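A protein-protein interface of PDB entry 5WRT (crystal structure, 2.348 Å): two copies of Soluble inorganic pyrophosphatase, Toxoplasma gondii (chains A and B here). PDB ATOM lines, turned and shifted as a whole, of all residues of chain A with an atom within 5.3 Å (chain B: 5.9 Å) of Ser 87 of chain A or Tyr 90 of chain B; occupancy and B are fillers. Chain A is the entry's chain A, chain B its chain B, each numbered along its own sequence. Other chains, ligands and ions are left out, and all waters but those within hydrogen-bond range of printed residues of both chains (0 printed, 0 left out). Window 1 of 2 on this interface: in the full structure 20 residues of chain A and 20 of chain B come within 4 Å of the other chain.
The backbone NH (N) of Tyr 85 of chain A lies within hydrogen-bond range of the backbone carbonyl oxygen (O) of Arg 58 of chain A, at 2.9 Å.
O of Thr 88 of chain A is in hydrogen-bond range of NE1 of Trp 190 of chain A (2.7 Å).
The backbone carbonyl oxygen (O) of Tyr 90 of chain B lies within hydrogen-bond range of the side-chain amino group (NZ) of Lys 55 of chain B (3.0 Å).
The backbone NH of Lys 55 of chain B sits at hydrogen-bond distance from the side-chain amide oxygen of Asn 92 of chain B (3.0 Å).
The backbone NH (N) of Asn 56 of chain B lies within hydrogen-bond range of the backbone carbonyl oxygen (O) of Leu 89 of chain B (2.7 Å).
O of Thr 88 of chain B sits at hydrogen-bond distance from NE1 of Trp 190 of chain B (2.7 Å).
Of the 12 printed residues of chain A, 8 touch a printed residue of chain B.
Printed residues of chain A that touch a printed residue of chain B: Arg 58, Ala 86, Ser 87, Thr 88, Trp 193, Tyr 194, Leu 196 and Pro 197.
Of the 12 printed residues of chain B, 8 touch a printed residue of chain A.
Hydrophobic or aromatic side chains of chain B that line the printed part of chain A: Ala 86, Tyr 90 and Trp 91.
The guanidinium group of Arg 58 of chain A lies within hydrogen-bond range of the backbone carbonyl oxygen of Ala 86 of chain B (3.1 Å).
The guanidinium group (NH1) of Arg 58 of chain B is in hydrogen-bond range of the backbone carbonyl oxygen (O) of Ala 86 of chain A (3.1 Å).
The backbone carbonyl oxygen (O) of Ala 86 of chain A is in hydrogen-bond range of the side-chain hydroxyl (OG1) of Thr 88 of chain B, 2.7 Å away.
The backbone NH (N) of Thr 88 of chain B is in hydrogen-bond range of the side-chain hydroxyl (OG) of Ser 87 of chain A (2.9 Å).
The side-chain hydroxyl of Tyr 90 of chain B is in hydrogen-bond range of the side-chain hydroxyl of Ser 87 of chain A, 2.6 Å away.
The side-chain hydroxyl of Thr 88 of chain A is in hydrogen-bond range of the backbone carbonyl oxygen of Ala 86 of chain B, at 2.8 Å.
The backbone NH of Thr 88 of chain A sits at hydrogen-bond distance from the side-chain hydroxyl of Ser 87 of chain B, 3.1 Å away.
The guanidinium group (NH2) of Arg 58 of chain A sits close to the guanidinium group (NH2) of Arg 58 of chain B (3.4 Å).
Arg 58 of chain B touches its own counterpart, Arg 58 of chain A.
Arg 58 of chain A touches Ala 86 of chain B, and with the chains exchanged Ala 86 of chain A touches Arg 58 of chain B.
Ala 86 of chain A touches Thr 88 of chain B, and with the chains exchanged Thr 88 of chain A touches Ala 86 of chain B.
Ser 87 of chain A touches Thr 88 of chain B, and with the chains exchanged Thr 88 of chain A touches Ser 87 of chain B.
7 positions are printed for both chains.
Of the 18 pairs that touch across the chains among the printed residues, 8 have their exchanged pair printed and touching as well.
Among the printed residues, pairs that only touch across the chains: Trp 193 of chain A with Tyr 90 of chain B, Pro 197 of chain A with Asn 56 of chain B, Ser 87 of chain A with Ser 87 of chain B, Tyr 194 of chain A with Tyr 90 of chain B, Leu 196 of chain A with Asn 56 of chain B, Pro 197 of chain A with Tyr 90 of chain B, Pro 197 of chain A with Thr 88 of chain B, Trp 193 of chain A with Trp 91 of chain B, Leu 196 of chain A with Lys 55 of chain B and Leu 196 of chain A with Tyr 90 of chain B.
Tyr 85 of chain A touches none of the printed residues of chain B.
Of the printed residues of chain B, Ala 86 of chain A touches Arg 58 and Thr 88.
Of chain B, only Ser 87 (3.4 Å), Thr 88 (2.9 Å) and Tyr 90 (2.6 Å) come within 4 Å of Ser 87 of chain A.
Leu 89 of chain A touches none of the printed residues of chain B.
Of the printed residues of chain B, Trp 193 of chain A touches Tyr 90 (3.2 Å) and Trp 91 (3.8 Å).
Of the printed residues of chain A, Lys 55 of chain B touches Leu 196 (3.8 Å).
Printed residues of chain A within 4 Å of Ser 87 of chain B: Ser 87 and Thr 88.
Of the printed residues of chain A, Thr 88 of chain B touches Ala 86, Ser 87 and Pro 197.
Of chain A, only Ser 87, Trp 193, Tyr 194, Leu 196 and Pro 197 come within 4 Å of Tyr 90 of chain B.
The nearest residue of chain B that does not touch Ser 87 of chain A is Ala 86 of chain B (4.2 Å).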
ATOM      1  N   THR A  57      16.467 -32.806  -8.968  1.00  0.00           N
ATOM      2  CA  THR A  57      15.459 -32.639 -10.006  1.00  0.00           C
ATOM      3  C   THR A  57      14.210 -32.026  -9.385  1.00  0.00           C
ATOM      4  O   THR A  57      14.101 -31.887  -8.163  1.00  0.00           O
ATOM      5  CB  THR A  57      15.107 -33.965 -10.700  1.00  0.00           C
ATOM      6  OG1 THR A  57      14.446 -34.836  -9.774  1.00  0.00           O
ATOM      7  CG2 THR A  57      16.358 -34.645 -11.243  1.00  0.00           C
ATOM      8  N   ARG A  58      13.254 -31.651 -10.237  1.00  0.00           N
ATOM      9  CA  ARG A  58      12.058 -30.980  -9.749  1.00  0.00           C
ATOM     10  C   ARG A  58      10.765 -31.448 -10.407  1.00  0.00           C
ATOM     11  O   ARG A  58       9.702 -30.927 -10.058  1.00  0.00           O
ATOM     12  CB  ARG A  58      12.188 -29.451  -9.874  1.00  0.00           C
ATOM     13  CG  ARG A  58      12.221 -28.882 -11.270  1.00  0.00           C
ATOM     14  CD  ARG A  58      12.030 -27.377 -11.180  1.00  0.00           C
ATOM     15  NE  ARG A  58      12.169 -26.707 -12.468  1.00  0.00           N
ATOM     16  CZ  ARG A  58      13.068 -25.760 -12.719  1.00  0.00           C
ATOM     17  NH1 ARG A  58      13.905 -25.370 -11.766  1.00  0.00           N
ATOM     18  NH2 ARG A  58      13.126 -25.200 -13.919  1.00  0.00           N
ATOM     19  N   TYR A  85       7.545 -29.282  -9.156  1.00  0.00           N
ATOM     20  CA  TYR A  85       7.690 -28.466  -7.962  1.00  0.00           C
ATOM     21  C   TYR A  85       8.297 -27.120  -8.339  1.00  0.00           C
ATOM     22  O   TYR A  85       9.038 -26.999  -9.318  1.00  0.00           O
ATOM     23  CB  TYR A  85       8.560 -29.172  -6.922  1.00  0.00           C
ATOM     24  CG  TYR A  85       7.876 -30.346  -6.257  1.00  0.00           C
ATOM     25  CD1 TYR A  85       6.584 -30.229  -5.760  1.00  0.00           C
ATOM     26  CD2 TYR A  85       8.520 -31.568  -6.124  1.00  0.00           C
ATOM     27  CE1 TYR A  85       5.951 -31.293  -5.152  1.00  0.00           C
ATOM     28  CE2 TYR A  85       7.895 -32.642  -5.516  1.00  0.00           C
ATOM     29  CZ  TYR A  85       6.610 -32.499  -5.033  1.00  0.00           C
ATOM     30  OH  TYR A  85       5.980 -33.562  -4.427  1.00  0.00           O
ATOM     31  N   ALA A  86       7.976 -26.095  -7.546  1.00  0.00           N
ATOM     32  CA  ALA A  86       8.510 -24.768  -7.818  1.00  0.00           C
ATOM     33  C   ALA A  86      10.008 -24.688  -7.571  1.00  0.00           C
ATOM     34  O   ALA A  86      10.661 -23.772  -8.082  1.00  0.00           O
ATOM     35  CB  ALA A  86       7.786 -23.724  -6.967  1.00  0.00           C
ATOM     36  N   SER A  87      10.566 -25.624  -6.808  1.00  0.00           N
ATOM     37  CA  SER A  87      11.977 -25.621  -6.463  1.00  0.00           C
ATOM     38  C   SER A  87      12.563 -27.007  -6.685  1.00  0.00           C
ATOM     39  O   SER A  87      11.853 -28.016  -6.637  1.00  0.00           O
ATOM     40  CB  SER A  87      12.190 -25.190  -5.009  1.00  0.00           C
ATOM     41  OG  SER A  87      11.929 -23.806  -4.853  1.00  0.00           O
ATOM     42  N   THR A  88      13.867 -27.043  -6.947  1.00  0.00           N
ATOM     43  CA  THR A  88      14.562 -28.313  -7.097  1.00  0.00           C
ATOM     44  C   THR A  88      14.712 -29.003  -5.745  1.00  0.00           C
ATOM     45  O   THR A  88      15.056 -28.374  -4.740  1.00  0.00           O
ATOM     46  CB  THR A  88      15.936 -28.094  -7.737  1.00  0.00           C
ATOM     47  OG1 THR A  88      15.772 -27.605  -9.075  1.00  0.00           O
ATOM     48  CG2 THR A  88      16.728 -29.387  -7.777  1.00  0.00           C
ATOM     49  N   LEU A  89      14.431 -30.305  -5.724  1.00  0.00           N
ATOM     50  CA  LEU A  89      14.652 -31.118  -4.536  1.00  0.00           C
ATOM     51  C   LEU A  89      16.102 -31.582  -4.502  1.00  0.00           C
ATOM     52  O   LEU A  89      16.606 -32.138  -5.482  1.00  0.00           O
ATOM     53  CB  LEU A  89      13.702 -32.315  -4.533  1.00  0.00           C
ATOM     54  CG  LEU A  89      13.440 -33.041  -3.212  1.00  0.00           C
ATOM     55  CD1 LEU A  89      13.332 -32.063  -2.055  1.00  0.00           C
ATOM     56  CD2 LEU A  89      12.170 -33.859  -3.331  1.00  0.00           C
ATOM     57  N   TRP A 190      12.835 -26.912   3.205  1.00  0.00           N
ATOM     58  CA  TRP A 190      12.377 -27.183   1.847  1.00  0.00           C
ATOM     59  C   TRP A 190      10.886 -27.490   1.828  1.00  0.00           C
ATOM     60  O   TRP A 190      10.123 -26.885   1.067  1.00  0.00           O
ATOM     61  CB  TRP A 190      13.170 -28.342   1.241  1.00  0.00           C
ATOM     62  CG  TRP A 190      13.094 -28.392  -0.255  1.00  0.00           C
ATOM     63  CD1 TRP A 190      14.020 -27.915  -1.138  1.00  0.00           C
ATOM     64  CD2 TRP A 190      12.030 -28.937  -1.046  1.00  0.00           C
ATOM     65  NE1 TRP A 190      13.601 -28.133  -2.427  1.00  0.00           N
ATOM     66  CE2 TRP A 190      12.381 -28.757  -2.399  1.00  0.00           C
ATOM     67  CE3 TRP A 190      10.816 -29.561  -0.743  1.00  0.00           C
ATOM     68  CZ2 TRP A 190      11.563 -29.180  -3.447  1.00  0.00           C
ATOM     69  CZ3 TRP A 190      10.005 -29.979  -1.784  1.00  0.00           C
ATOM     70  CH2 TRP A 190      10.382 -29.786  -3.118  1.00  0.00           C
ATOM     71  N   TRP A 193       8.424 -24.494   2.820  1.00  0.00           N
ATOM     72  CA  TRP A 193       8.264 -23.342   1.945  1.00  0.00           C
ATOM     73  C   TRP A 193       7.881 -23.684   0.509  1.00  0.00           C
ATOM     74  O   TRP A 193       7.484 -22.777  -0.230  1.00  0.00           O
ATOM     75  CB  TRP A 193       9.562 -22.517   1.926  1.00  0.00           C
ATOM     76  CG  TRP A 193       9.848 -21.802   3.213  1.00  0.00           C
ATOM     77  CD1 TRP A 193      10.708 -22.196   4.198  1.00  0.00           C
ATOM     78  CD2 TRP A 193       9.280 -20.561   3.649  1.00  0.00           C
ATOM     79  NE1 TRP A 193      10.705 -21.281   5.223  1.00  0.00           N
ATOM     80  CE2 TRP A 193       9.837 -20.266   4.911  1.00  0.00           C
ATOM     81  CE3 TRP A 193       8.352 -19.671   3.098  1.00  0.00           C
ATOM     82  CZ2 TRP A 193       9.497 -19.121   5.629  1.00  0.00           C
ATOM     83  CZ3 TRP A 193       8.017 -18.535   3.812  1.00  0.00           C
ATOM     84  CH2 TRP A 193       8.588 -18.270   5.064  1.00  0.00           C
ATOM     85  N   TYR A 194       7.980 -24.948   0.091  1.00  0.00           N
ATOM     86  CA  TYR A 194       7.945 -25.247  -1.341  1.00  0.00           C
ATOM     87  C   TYR A 194       6.578 -25.029  -1.985  1.00  0.00           C
ATOM     88  O   TYR A 194       6.495 -24.984  -3.216  1.00  0.00           O
ATOM     89  CB  TYR A 194       8.419 -26.679  -1.603  1.00  0.00           C
ATOM     90  CG  TYR A 194       7.405 -27.759  -1.305  1.00  0.00           C
ATOM     91  CD1 TYR A 194       6.922 -27.949  -0.019  1.00  0.00           C
ATOM     92  CD2 TYR A 194       6.942 -28.596  -2.312  1.00  0.00           C
ATOM     93  CE1 TYR A 194       6.000 -28.941   0.257  1.00  0.00           C
ATOM     94  CE2 TYR A 194       6.021 -29.591  -2.047  1.00  0.00           C
ATOM     95  CZ  TYR A 194       5.553 -29.759  -0.759  1.00  0.00           C
ATOM     96  OH  TYR A 194       4.635 -30.749  -0.486  1.00  0.00           O
ATOM     97  N   LEU A 196       4.636 -22.310  -1.170  1.00  0.00           N
ATOM     98  CA  LEU A 196       4.301 -20.888  -1.137  1.00  0.00           C
ATOM     99  C   LEU A 196       4.055 -20.316  -2.526  1.00  0.00           C
ATOM    100  O   LEU A 196       3.069 -19.579  -2.697  1.00  0.00           O
ATOM    101  CB  LEU A 196       5.385 -20.101  -0.395  1.00  0.00           C
ATOM    102  CG  LEU A 196       4.982 -18.654  -0.088  1.00  0.00           C
ATOM    103  CD1 LEU A 196       3.976 -18.606   1.055  1.00  0.00           C
ATOM    104  CD2 LEU A 196       6.197 -17.792   0.226  1.00  0.00           C
ATOM    105  N   PRO A 197       4.885 -20.579  -3.544  1.00  0.00           N
ATOM    106  CA  PRO A 197       4.581 -20.007  -4.865  1.00  0.00           C
ATOM    107  C   PRO A 197       3.352 -20.615  -5.514  1.00  0.00           C
ATOM    108  O   PRO A 197       2.633 -19.910  -6.231  1.00  0.00           O
ATOM    109  CB  PRO A 197       5.849 -20.300  -5.683  1.00  0.00           C
ATOM    110  CG  PRO A 197       6.892 -20.690  -4.685  1.00  0.00           C
ATOM    111  CD  PRO A 197       6.154 -21.328  -3.564  1.00  0.00           C
ATOM    112  N   LYS B  55       9.381 -11.795  -4.614  1.00  0.00           N
ATOM    113  CA  LYS B  55       8.949 -12.967  -3.866  1.00  0.00           C
ATOM    114  C   LYS B  55       8.245 -13.964  -4.780  1.00  0.00           C
ATOM    115  O   LYS B  55       7.404 -13.584  -5.600  1.00  0.00           O
ATOM    116  CB  LYS B  55       8.016 -12.527  -2.734  1.00  0.00           C
ATOM    117  CG  LYS B  55       7.312 -13.645  -1.993  1.00  0.00           C
ATOM    118  CD  LYS B  55       6.287 -13.072  -1.022  1.00  0.00           C
ATOM    119  CE  LYS B  55       6.004 -14.025   0.126  1.00  0.00           C
ATOM    120  NZ  LYS B  55       7.090 -14.016   1.150  1.00  0.00           N
ATOM    121  N   ASN B  56       8.633 -15.239  -4.661  1.00  0.00           N
ATOM    122  CA  ASN B  56       8.011 -16.355  -5.378  1.00  0.00           C
ATOM    123  C   ASN B  56       8.339 -16.345  -6.869  1.00  0.00           C
ATOM    124  O   ASN B  56       7.513 -16.742  -7.694  1.00  0.00           O
ATOM    125  CB  ASN B  56       6.492 -16.390  -5.168  1.00  0.00           C
ATOM    126  CG  ASN B  56       6.105 -16.913  -3.799  1.00  0.00           C
ATOM    127  OD1 ASN B  56       6.838 -17.691  -3.187  1.00  0.00           O
ATOM    128  ND2 ASN B  56       4.947 -16.484  -3.308  1.00  0.00           N
ATOM    129  N   THR B  57       9.546 -15.916  -7.229  1.00  0.00           N
ATOM    130  CA  THR B  57      10.017 -15.981  -8.605  1.00  0.00           C
ATOM    131  C   THR B  57      11.371 -16.677  -8.644  1.00  0.00           C
ATOM    132  O   THR B  57      11.979 -16.967  -7.609  1.00  0.00           O
ATOM    133  CB  THR B  57      10.113 -14.590  -9.253  1.00  0.00           C
ATOM    134  OG1 THR B  57      11.137 -13.821  -8.607  1.00  0.00           O
ATOM    135  CG2 THR B  57       8.779 -13.854  -9.164  1.00  0.00           C
ATOM    136  N   ARG B  58      11.845 -16.929  -9.863  1.00  0.00           N
ATOM    137  CA  ARG B  58      13.044 -17.732 -10.060  1.00  0.00           C
ATOM    138  C   ARG B  58      14.015 -17.164 -11.084  1.00  0.00           C
ATOM    139  O   ARG B  58      15.140 -17.666 -11.179  1.00  0.00           O
ATOM    140  CB  ARG B  58      12.618 -19.145 -10.497  1.00  0.00           C
ATOM    141  CG  ARG B  58      13.658 -20.233 -10.384  1.00  0.00           C
ATOM    142  CD  ARG B  58      13.017 -21.609 -10.556  1.00  0.00           C
ATOM    143  NE  ARG B  58      12.339 -21.758 -11.844  1.00  0.00           N
ATOM    144  CZ  ARG B  58      11.411 -22.677 -12.095  1.00  0.00           C
ATOM    145  NH1 ARG B  58      11.050 -23.532 -11.146  1.00  0.00           N
ATOM    146  NH2 ARG B  58      10.843 -22.745 -13.292  1.00  0.00           N
ATOM    147  N   ALA B  86      17.985 -22.547  -9.608  1.00  0.00           N
ATOM    148  CA  ALA B  86      17.386 -23.875  -9.662  1.00  0.00           C
ATOM    149  C   ALA B  86      16.126 -23.969  -8.811  1.00  0.00           C
ATOM    150  O   ALA B  86      15.302 -24.861  -9.043  1.00  0.00           O
ATOM    151  CB  ALA B  86      18.396 -24.928  -9.220  1.00  0.00           C
ATOM    152  N   SER B  87      15.947 -23.057  -7.858  1.00  0.00           N
ATOM    153  CA  SER B  87      14.813 -23.075  -6.949  1.00  0.00           C
ATOM    154  C   SER B  87      14.183 -21.693  -6.881  1.00  0.00           C
ATOM    155  O   SER B  87      14.852 -20.674  -7.078  1.00  0.00           O
ATOM    156  CB  SER B  87      15.233 -23.520  -5.543  1.00  0.00           C
ATOM    157  OG  SER B  87      15.544 -24.901  -5.524  1.00  0.00           O
ATOM    158  N   THR B  88      12.885 -21.669  -6.590  1.00  0.00           N
ATOM    159  CA  THR B  88      12.172 -20.410  -6.437  1.00  0.00           C
ATOM    160  C   THR B  88      12.581 -19.718  -5.142  1.00  0.00           C
ATOM    161  O   THR B  88      12.680 -20.349  -4.085  1.00  0.00           O
ATOM    162  CB  THR B  88      10.661 -20.651  -6.452  1.00  0.00           C
ATOM    163  OG1 THR B  88      10.270 -21.158  -7.733  1.00  0.00           O
ATOM    164  CG2 THR B  88       9.907 -19.362  -6.180  1.00  0.00           C
ATOM    165  N   LEU B  89      12.826 -18.413  -5.231  1.00  0.00           N
ATOM    166  CA  LEU B  89      13.114 -17.608  -4.053  1.00  0.00           C
ATOM    167  C   LEU B  89      11.804 -17.171  -3.407  1.00  0.00           C
ATOM    168  O   LEU B  89      10.934 -16.601  -4.072  1.00  0.00           O
ATOM    169  CB  LEU B  89      13.960 -16.397  -4.443  1.00  0.00           C
ATOM    170  CG  LEU B  89      14.762 -15.669  -3.364  1.00  0.00           C
ATOM    171  CD1 LEU B  89      15.378 -16.649  -2.375  1.00  0.00           C
ATOM    172  CD2 LEU B  89      15.841 -14.827  -4.023  1.00  0.00           C
ATOM    173  N   TYR B  90      11.670 -17.429  -2.109  1.00  0.00           N
ATOM    174  CA  TYR B  90      10.411 -17.234  -1.401  1.00  0.00           C
ATOM    175  C   TYR B  90      10.302 -15.871  -0.730  1.00  0.00           C
ATOM    176  O   TYR B  90       9.382 -15.659   0.066  1.00  0.00           O
ATOM    177  CB  TYR B  90      10.219 -18.343  -0.362  1.00  0.00           C
ATOM    178  CG  TYR B  90      10.357 -19.738  -0.934  1.00  0.00           C
ATOM    179  CD1 TYR B  90       9.427 -20.228  -1.843  1.00  0.00           C
ATOM    180  CD2 TYR B  90      11.419 -20.561  -0.578  1.00  0.00           C
ATOM    181  CE1 TYR B  90       9.545 -21.497  -2.373  1.00  0.00           C
ATOM    182  CE2 TYR B  90      11.546 -21.835  -1.108  1.00  0.00           C
ATOM    183  CZ  TYR B  90      10.604 -22.296  -2.005  1.00  0.00           C
ATOM    184  OH  TYR B  90      10.713 -23.559  -2.540  1.00  0.00           O
ATOM    185  N   TRP B  91      11.209 -14.945  -1.028  1.00  0.00           N
ATOM    186  CA  TRP B  91      11.188 -13.624  -0.423  1.00  0.00           C
ATOM    187  C   TRP B  91      11.645 -12.600  -1.448  1.00  0.00           C
ATOM    188  O   TRP B  91      12.410 -12.918  -2.363  1.00  0.00           O
ATOM    189  CB  TRP B  91      12.087 -13.560   0.818  1.00  0.00           C
ATOM    190  CG  TRP B  91      11.845 -14.672   1.787  1.00  0.00           C
ATOM    191  CD1 TRP B  91      10.984 -14.668   2.846  1.00  0.00           C
ATOM    192  CD2 TRP B  91      12.454 -15.970   1.769  1.00  0.00           C
ATOM    193  NE1 TRP B  91      11.029 -15.877   3.497  1.00  0.00           N
ATOM    194  CE2 TRP B  91      11.922 -16.695   2.853  1.00  0.00           C
ATOM    195  CE3 TRP B  91      13.398 -16.586   0.943  1.00  0.00           C
ATOM    196  CZ2 TRP B  91      12.306 -18.005   3.135  1.00  0.00           C
ATOM    197  CZ3 TRP B  91      13.779 -17.888   1.225  1.00  0.00           C
ATOM    198  CH2 TRP B  91      13.233 -18.582   2.312  1.00  0.00           C
ATOM    199  N   ASN B  92      11.157 -11.370  -1.300  1.00  0.00           N
ATOM    200  CA  ASN B  92      11.655 -10.279  -2.127  1.00  0.00           C
ATOM    201  C   ASN B  92      13.150 -10.104  -1.900  1.00  0.00           C
ATOM    202  O   ASN B  92      13.630 -10.122  -0.763  1.00  0.00           O
ATOM    203  CB  ASN B  92      10.914  -8.979  -1.816  1.00  0.00           C
ATOM    204  CG  ASN B  92       9.413  -9.102  -2.003  1.00  0.00           C
ATOM    205  OD1 ASN B  92       8.925  -9.226  -3.127  1.00  0.00           O
ATOM    206  ND2 ASN B  92       8.673  -9.055  -0.901  1.00  0.00           N
ATOM    207  N   TRP B 190      18.006 -21.893   2.171  1.00  0.00           N
ATOM    208  CA  TRP B 190      17.857 -21.616   0.746  1.00  0.00           C
ATOM    209  C   TRP B 190      19.204 -21.288   0.116  1.00  0.00           C
ATOM    210  O   TRP B 190      19.585 -21.870  -0.906  1.00  0.00           O
ATOM    211  CB  TRP B 190      16.868 -20.472   0.522  1.00  0.00           C
ATOM    212  CG  TRP B 190      16.338 -20.409  -0.882  1.00  0.00           C
ATOM    213  CD1 TRP B 190      15.149 -20.905  -1.332  1.00  0.00           C
ATOM    214  CD2 TRP B 190      16.983 -19.820  -2.019  1.00  0.00           C
ATOM    215  NE1 TRP B 190      15.013 -20.657  -2.678  1.00  0.00           N
ATOM    216  CE2 TRP B 190      16.125 -19.993  -3.124  1.00  0.00           C
ATOM    217  CE3 TRP B 190      18.202 -19.161  -2.209  1.00  0.00           C
ATOM    218  CZ2 TRP B 190      16.446 -19.533  -4.398  1.00  0.00           C
ATOM    219  CZ3 TRP B 190      18.519 -18.706  -3.477  1.00  0.00           C
ATOM    220  CH2 TRP B 190      17.645 -18.894  -4.555  1.00  0.00           C
